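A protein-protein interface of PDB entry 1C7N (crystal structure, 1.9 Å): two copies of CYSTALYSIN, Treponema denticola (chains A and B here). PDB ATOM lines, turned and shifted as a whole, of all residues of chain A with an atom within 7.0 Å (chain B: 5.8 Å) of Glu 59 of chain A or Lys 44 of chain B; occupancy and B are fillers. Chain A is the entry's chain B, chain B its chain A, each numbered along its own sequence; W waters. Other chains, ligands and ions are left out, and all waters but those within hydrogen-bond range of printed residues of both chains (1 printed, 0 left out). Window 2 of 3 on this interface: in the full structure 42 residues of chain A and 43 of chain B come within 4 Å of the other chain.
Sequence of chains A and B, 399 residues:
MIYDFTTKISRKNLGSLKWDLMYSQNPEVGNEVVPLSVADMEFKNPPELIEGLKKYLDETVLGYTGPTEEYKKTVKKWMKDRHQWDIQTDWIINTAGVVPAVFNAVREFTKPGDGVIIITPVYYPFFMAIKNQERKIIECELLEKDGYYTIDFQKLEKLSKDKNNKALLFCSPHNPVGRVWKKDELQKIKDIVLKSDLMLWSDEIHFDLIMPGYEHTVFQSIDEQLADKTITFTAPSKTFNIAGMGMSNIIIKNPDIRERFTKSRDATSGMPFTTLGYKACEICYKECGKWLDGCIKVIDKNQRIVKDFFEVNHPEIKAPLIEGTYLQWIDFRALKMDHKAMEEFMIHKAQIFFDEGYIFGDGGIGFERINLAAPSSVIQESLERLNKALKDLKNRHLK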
ATOM      1  N   GLY A  52      16.147   0.930  23.019  1.00  0.00           N
ATOM      2  CA  GLY A  52      16.848   1.354  24.218  1.00  0.00           C
ATOM      3  C   GLY A  52      18.351   1.466  24.010  1.00  0.00           C
ATOM      4  O   GLY A  52      18.978   2.412  24.479  1.00  0.00           O
ATOM      5  N   LYS A  54      19.906   1.966  21.134  1.00  0.00           N
ATOM      6  CA  LYS A  54      20.168   3.069  20.215  1.00  0.00           C
ATOM      7  C   LYS A  54      20.144   4.381  20.994  1.00  0.00           C
ATOM      8  O   LYS A  54      21.008   5.240  20.818  1.00  0.00           O
ATOM      9  CB  LYS A  54      19.117   3.111  19.090  1.00  0.00           C
ATOM     10  CG  LYS A  54      19.267   1.992  18.064  1.00  0.00           C
ATOM     11  CD  LYS A  54      18.453   2.244  16.794  1.00  0.00           C
ATOM     12  CE  LYS A  54      16.964   2.140  17.056  1.00  0.00           C
ATOM     13  NZ  LYS A  54      16.164   2.307  15.810  1.00  0.00           N
ATOM     14  N   LYS A  55      19.154   4.519  21.868  1.00  0.00           N
ATOM     15  CA  LYS A  55      19.009   5.712  22.686  1.00  0.00           C
ATOM     16  C   LYS A  55      20.225   5.889  23.600  1.00  0.00           C
ATOM     17  O   LYS A  55      20.763   6.992  23.740  1.00  0.00           O
ATOM     18  CB  LYS A  55      17.741   5.611  23.536  1.00  0.00           C
ATOM     19  CG  LYS A  55      17.524   6.801  24.452  1.00  0.00           C
ATOM     20  CD  LYS A  55      16.310   6.623  25.344  1.00  0.00           C
ATOM     21  CE  LYS A  55      16.145   7.824  26.262  1.00  0.00           C
ATOM     22  NZ  LYS A  55      15.051   7.627  27.249  1.00  0.00           N
ATOM     23  N   TYR A  56      20.654   4.791  24.215  1.00  0.00           N
ATOM     24  CA  TYR A  56      21.797   4.814  25.118  1.00  0.00           C
ATOM     25  C   TYR A  56      23.058   5.274  24.378  1.00  0.00           C
ATOM     26  O   TYR A  56      23.886   5.997  24.934  1.00  0.00           O
ATOM     27  CB  TYR A  56      22.021   3.422  25.715  1.00  0.00           C
ATOM     28  CG  TYR A  56      23.029   3.398  26.841  1.00  0.00           C
ATOM     29  CD1 TYR A  56      24.118   2.531  26.811  1.00  0.00           C
ATOM     30  CD2 TYR A  56      22.884   4.234  27.942  1.00  0.00           C
ATOM     31  CE1 TYR A  56      25.044   2.496  27.859  1.00  0.00           C
ATOM     32  CE2 TYR A  56      23.798   4.211  28.993  1.00  0.00           C
ATOM     33  CZ  TYR A  56      24.874   3.340  28.947  1.00  0.00           C
ATOM     34  OH  TYR A  56      25.771   3.311  29.988  1.00  0.00           O
ATOM     35  N   LEU A  57      23.192   4.854  23.123  1.00  0.00           N
ATOM     36  CA  LEU A  57      24.343   5.222  22.309  1.00  0.00           C
ATOM     37  C   LEU A  57      24.442   6.721  22.049  1.00  0.00           C
ATOM     38  O   LEU A  57      25.546   7.266  21.965  1.00  0.00           O
ATOM     39  CB  LEU A  57      24.312   4.466  20.978  1.00  0.00           C
ATOM     40  CG  LEU A  57      24.644   2.975  21.098  1.00  0.00           C
ATOM     41  CD1 LEU A  57      24.426   2.270  19.764  1.00  0.00           C
ATOM     42  CD2 LEU A  57      26.086   2.819  21.567  1.00  0.00           C
ATOM     43  N   ASP A  58      23.296   7.388  21.922  1.00  0.00           N
ATOM     44  CA  ASP A  58      23.288   8.830  21.685  1.00  0.00           C
ATOM     45  C   ASP A  58      23.716   9.594  22.930  1.00  0.00           C
ATOM     46  O   ASP A  58      24.113  10.753  22.839  1.00  0.00           O
ATOM     47  CB  ASP A  58      21.890   9.329  21.305  1.00  0.00           C
ATOM     48  CG  ASP A  58      21.415   8.816  19.964  1.00  0.00           C
ATOM     49  OD1 ASP A  58      22.163   8.934  18.969  1.00  0.00           O
ATOM     50  OD2 ASP A  58      20.276   8.309  19.903  1.00  0.00           O
ATOM     51  N   GLU A  59      23.644   8.945  24.089  1.00  0.00           N
ATOM     52  CA  GLU A  59      23.967   9.605  25.348  1.00  0.00           C
ATOM     53  C   GLU A  59      25.231   9.184  26.093  1.00  0.00           C
ATOM     54  O   GLU A  59      25.659   9.878  27.012  1.00  0.00           O
ATOM     55  CB  GLU A  59      22.777   9.464  26.304  1.00  0.00           C
ATOM     56  CG  GLU A  59      21.532  10.227  25.870  1.00  0.00           C
ATOM     57  CD  GLU A  59      20.285   9.361  25.841  1.00  0.00           C
ATOM     58  OE1 GLU A  59      19.989   8.697  26.858  1.00  0.00           O
ATOM     59  OE2 GLU A  59      19.593   9.355  24.799  1.00  0.00           O
ATOM     60  N   THR A  60      25.842   8.073  25.703  1.00  0.00           N
ATOM     61  CA  THR A  60      27.014   7.589  26.422  1.00  0.00           C
ATOM     62  C   THR A  60      28.356   7.696  25.708  1.00  0.00           C
ATOM     63  O   THR A  60      28.429   7.997  24.521  1.00  0.00           O
ATOM     64  CB  THR A  60      26.826   6.115  26.812  1.00  0.00           C
ATOM     65  OG1 THR A  60      25.443   5.874  27.084  1.00  0.00           O
ATOM     66  CG2 THR A  60      27.640   5.778  28.056  1.00  0.00           C
ATOM     67  N   VAL A  61      29.411   7.445  26.477  1.00  0.00           N
ATOM     68  CA  VAL A  61      30.788   7.432  26.002  1.00  0.00           C
ATOM     69  C   VAL A  61      31.205   5.975  26.194  1.00  0.00           C
ATOM     70  O   VAL A  61      31.064   5.430  27.290  1.00  0.00           O
ATOM     71  CB  VAL A  61      31.681   8.357  26.856  1.00  0.00           C
ATOM     72  CG1 VAL A  61      33.153   8.106  26.542  1.00  0.00           C
ATOM     73  CG2 VAL A  61      31.322   9.809  26.576  1.00  0.00           C
ATOM     74  N   LEU A  62      31.718   5.346  25.142  1.00  0.00           N
ATOM     75  CA  LEU A  62      32.087   3.932  25.213  1.00  0.00           C
ATOM     76  C   LEU A  62      33.420   3.605  25.891  1.00  0.00           C
ATOM     77  O   LEU A  62      34.172   2.762  25.404  1.00  0.00           O
ATOM     78  CB  LEU A  62      32.051   3.332  23.800  1.00  0.00           C
ATOM     79  CG  LEU A  62      30.705   3.515  23.085  1.00  0.00           C
ATOM     80  CD1 LEU A  62      30.797   3.030  21.636  1.00  0.00           C
ATOM     81  CD2 LEU A  62      29.622   2.757  23.836  1.00  0.00           C
ATOM     82  N   LYS A 279      23.939  -2.306  30.116  1.00  0.00           N
ATOM     83  CA  LYS A 279      22.708  -1.635  29.720  1.00  0.00           C
ATOM     84  C   LYS A 279      21.680  -2.581  29.094  1.00  0.00           C
ATOM     85  O   LYS A 279      20.483  -2.468  29.354  1.00  0.00           O
ATOM     86  CB  LYS A 279      23.019  -0.506  28.735  1.00  0.00           C
ATOM     87  CG  LYS A 279      21.799   0.309  28.332  1.00  0.00           C
ATOM     88  CD  LYS A 279      21.201   1.039  29.528  1.00  0.00           C
ATOM     89  CE  LYS A 279      20.080   1.971  29.096  1.00  0.00           C
ATOM     90  NZ  LYS A 279      19.512   2.712  30.262  1.00  0.00           N
ATOM     91  N   ASP B   4      32.927  16.969  17.079  1.00  0.00           N
ATOM     92  CA  ASP B   4      32.869  17.768  18.297  1.00  0.00           C
ATOM     93  C   ASP B   4      33.925  17.389  19.332  1.00  0.00           C
ATOM     94  O   ASP B   4      33.868  16.308  19.918  1.00  0.00           O
ATOM     95  CB  ASP B   4      31.474  17.637  18.920  1.00  0.00           C
ATOM     96  CG  ASP B   4      31.313  18.451  20.196  1.00  0.00           C
ATOM     97  OD1 ASP B   4      32.320  18.959  20.740  1.00  0.00           O
ATOM     98  OD2 ASP B   4      30.167  18.570  20.666  1.00  0.00           O
ATOM     99  N   ILE B   9      31.511  17.420  28.447  1.00  0.00           N
ATOM    100  CA  ILE B   9      30.556  16.403  28.873  1.00  0.00           C
ATOM    101  C   ILE B   9      30.761  16.000  30.327  1.00  0.00           C
ATOM    102  O   ILE B   9      31.787  16.303  30.932  1.00  0.00           O
ATOM    103  CB  ILE B   9      30.665  15.129  27.998  1.00  0.00           C
ATOM    104  CG1 ILE B   9      32.014  14.446  28.237  1.00  0.00           C
ATOM    105  CG2 ILE B   9      30.519  15.494  26.526  1.00  0.00           C
ATOM    106  CD1 ILE B   9      32.214  13.165  27.446  1.00  0.00           C
ATOM    107  N   LEU B  14      27.443   7.340  35.793  1.00  0.00           N
ATOM    108  CA  LEU B  14      27.162   6.674  34.523  1.00  0.00           C
ATOM    109  C   LEU B  14      27.949   5.368  34.395  1.00  0.00           C
ATOM    110  O   LEU B  14      28.017   4.778  33.321  1.00  0.00           O
ATOM    111  CB  LEU B  14      27.512   7.602  33.357  1.00  0.00           C
ATOM    112  CG  LEU B  14      26.413   8.486  32.758  1.00  0.00           C
ATOM    113  CD1 LEU B  14      25.536   9.089  33.840  1.00  0.00           C
ATOM    114  CD2 LEU B  14      27.071   9.573  31.921  1.00  0.00           C
ATOM    115  N   GLU B  42      37.425  12.008  26.980  1.00  0.00           N
ATOM    116  CA  GLU B  42      36.342  12.861  27.444  1.00  0.00           C
ATOM    117  C   GLU B  42      35.702  13.522  26.221  1.00  0.00           C
ATOM    118  O   GLU B  42      35.340  14.701  26.237  1.00  0.00           O
ATOM    119  CB  GLU B  42      36.879  13.912  28.416  1.00  0.00           C
ATOM    120  CG  GLU B  42      37.216  13.348  29.801  1.00  0.00           C
ATOM    121  CD  GLU B  42      36.047  12.588  30.427  1.00  0.00           C
ATOM    122  OE1 GLU B  42      34.931  13.142  30.477  1.00  0.00           O
ATOM    123  OE2 GLU B  42      36.243  11.440  30.879  1.00  0.00           O
ATOM    124  N   PHE B  43      35.584  12.732  25.159  1.00  0.00           N
ATOM    125  CA  PHE B  43      34.989  13.161  23.900  1.00  0.00           C
ATOM    126  C   PHE B  43      33.900  12.155  23.557  1.00  0.00           C
ATOM    127  O   PHE B  43      33.999  10.981  23.920  1.00  0.00           O
ATOM    128  CB  PHE B  43      36.016  13.108  22.761  1.00  0.00           C
ATOM    129  CG  PHE B  43      37.167  14.065  22.907  1.00  0.00           C
ATOM    130  CD1 PHE B  43      38.466  13.645  22.629  1.00  0.00           C
ATOM    131  CD2 PHE B  43      36.954  15.396  23.252  1.00  0.00           C
ATOM    132  CE1 PHE B  43      39.539  14.541  22.689  1.00  0.00           C
ATOM    133  CE2 PHE B  43      38.016  16.295  23.313  1.00  0.00           C
ATOM    134  CZ  PHE B  43      39.310  15.868  23.029  1.00  0.00           C
ATOM    135  N   LYS B  44      32.855  12.592  22.868  1.00  0.00           N
ATOM    136  CA  LYS B  44      31.850  11.629  22.455  1.00  0.00           C
ATOM    137  C   LYS B  44      32.570  10.811  21.376  1.00  0.00           C
ATOM    138  O   LYS B  44      33.532  11.285  20.760  1.00  0.00           O
ATOM    139  CB  LYS B  44      30.615  12.326  21.873  1.00  0.00           C
ATOM    140  CG  LYS B  44      29.613  12.838  22.921  1.00  0.00           C
ATOM    141  CD  LYS B  44      29.106  11.693  23.805  1.00  0.00           C
ATOM    142  CE  LYS B  44      27.698  11.951  24.358  1.00  0.00           C
ATOM    143  NZ  LYS B  44      27.596  13.147  25.245  1.00  0.00           N
ATOM    144  N   ASN B  45      32.128   9.582  21.158  1.00  0.00           N
ATOM    145  CA  ASN B  45      32.750   8.731  20.143  1.00  0.00           C
ATOM    146  C   ASN B  45      32.500   9.289  18.741  1.00  0.00           C
ATOM    147  O   ASN B  45      31.663  10.169  18.556  1.00  0.00           O
ATOM    148  CB  ASN B  45      32.202   7.313  20.273  1.00  0.00           C
ATOM    149  CG  ASN B  45      32.670   6.635  21.546  1.00  0.00           C
ATOM    150  OD1 ASN B  45      33.805   6.160  21.626  1.00  0.00           O
ATOM    151  ND2 ASN B  45      31.811   6.608  22.555  1.00  0.00           N
ATOM    152  N   PRO B  46      33.236   8.794  17.737  1.00  0.00           N
ATOM    153  CA  PRO B  46      33.041   9.290  16.372  1.00  0.00           C
ATOM    154  C   PRO B  46      31.583   9.149  15.938  1.00  0.00           C
ATOM    155  O   PRO B  46      30.958   8.115  16.163  1.00  0.00           O
ATOM    156  CB  PRO B  46      33.968   8.404  15.546  1.00  0.00           C
ATOM    157  CG  PRO B  46      35.053   8.058  16.512  1.00  0.00           C
ATOM    158  CD  PRO B  46      34.295   7.770  17.779  1.00  0.00           C
ATOM    159  N   ASN B 241      38.424   5.522  21.433  1.00  0.00           N
ATOM    160  CA  ASN B 241      37.740   5.619  22.720  1.00  0.00           C
ATOM    161  C   ASN B 241      36.638   4.571  22.909  1.00  0.00           C
ATOM    162  O   ASN B 241      35.526   4.896  23.346  1.00  0.00           O
ATOM    163  CB  ASN B 241      37.161   7.034  22.873  1.00  0.00           C
ATOM    164  CG  ASN B 241      36.700   7.336  24.284  1.00  0.00           C
ATOM    165  OD1 ASN B 241      37.131   6.700  25.243  1.00  0.00           O
ATOM    166  ND2 ASN B 241      35.831   8.332  24.420  1.00  0.00           N
ATOM    167  N   TRP B 291      37.837  11.618  11.807  1.00  0.00           N
ATOM    168  CA  TRP B 291      37.614  11.941  13.204  1.00  0.00           C
ATOM    169  C   TRP B 291      38.938  11.820  13.955  1.00  0.00           C
ATOM    170  O   TRP B 291      39.281  12.675  14.771  1.00  0.00           O
ATOM    171  CB  TRP B 291      36.571  11.000  13.813  1.00  0.00           C
ATOM    172  CG  TRP B 291      36.343  11.244  15.270  1.00  0.00           C
ATOM    173  CD1 TRP B 291      35.447  12.107  15.837  1.00  0.00           C
ATOM    174  CD2 TRP B 291      37.058  10.637  16.348  1.00  0.00           C
ATOM    175  NE1 TRP B 291      35.565  12.072  17.213  1.00  0.00           N
ATOM    176  CE2 TRP B 291      36.548  11.178  17.547  1.00  0.00           C
ATOM    177  CE3 TRP B 291      38.087   9.687  16.416  1.00  0.00           C
ATOM    178  CZ2 TRP B 291      37.034  10.799  18.803  1.00  0.00           C
ATOM    179  CZ3 TRP B 291      38.565   9.313  17.663  1.00  0.00           C
ATOM    180  CH2 TRP B 291      38.035   9.870  18.840  1.00  0.00           C
HETATM  181  O   HOH W   1      29.726   8.945  22.154  1.00  0.00           O
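The side-chain amide nitrogen (ND2) of Asn 45 of chain B lies close to the backbone NH (N) of Leu 62 of chain A (2.9 Å).
The backbone carbonyl oxygen (O) of Leu 62 of chain A lies close to the backbone carbonyl oxygen (O) of Asn 241 of chain B (3.3 Å).
O of Phe 43 of chain B is in hydrogen-bond range of ND2 of Asn 241 of chain B, at 3.3 Å.
O of Asn 241 of chain B lies close to OD1 of Asn 45 of chain B (2.7 Å).
O of Tyr 56 of chain A sits at hydrogen-bond distance from OG1 of Thr 60 of chain A (2.7 Å).
Glu 59 of chain A touches Lys 44 of chain B (O to CE, 3.9 Å).
CD of Lys 44 of chain B touches O of Thr 60 of chain A (3.8 Å).
Val 61 of chain A touches Ile 9 of chain B.
Phe 43 of chain B touches Val 61 of chain A (O to CG2, 3.9 Å).
Val 61 of chain A touches Asn 45 of chain B (CA to ND2, 3.7 Å).
CG1 of Val 61 of chain A touches ND2 of Asn 241 of chain B, 3.4 Å away.
Glu 59 of chain A touches one residue of chain B.
Printed residues of chain A within 4 Å of Lys 44 of chain B: Glu 59 (3.9 Å) and Thr 60 (3.8 Å).
Of the printed residues of chain A, Asn 45 of chain B touches Val 61 and Leu 62.
Printed residues of chain A within 4 Å of Asn 241 of chain B: Val 61 and Leu 62.
Printed residues of chain B within 4 Å of Val 61 of chain A: Ile 9, Phe 43, Asn 45 and Asn 241.
Of the printed residues of chain A, Phe 43 of chain B touches Val 61.
Lys 54 of chain A touches none of the printed residues of chain B.
Glu 42 of chain B touches none of the printed residues of chain A.
The nearest printed residue of chain A that does not touch Lys 44 of chain B is Val 61 of chain A (4.02 Å).
Hydrophobic or aromatic side chains of chain B within 4 Å of the printed part of chain A: Ile 9.
Among the printed residues, 8 pairs touch across the chains.
Among the printed residues, no Asp or Glu carboxylate lies within 4 Å of a Lys or Arg side-chain nitrogen of the other chain.
No position is printed for both chains.
Water W1 lies within hydrogen-bond range of N of Asn 45 of chain B (2.7 Å) and O of Thr 60 of chain A (2.9 Å).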
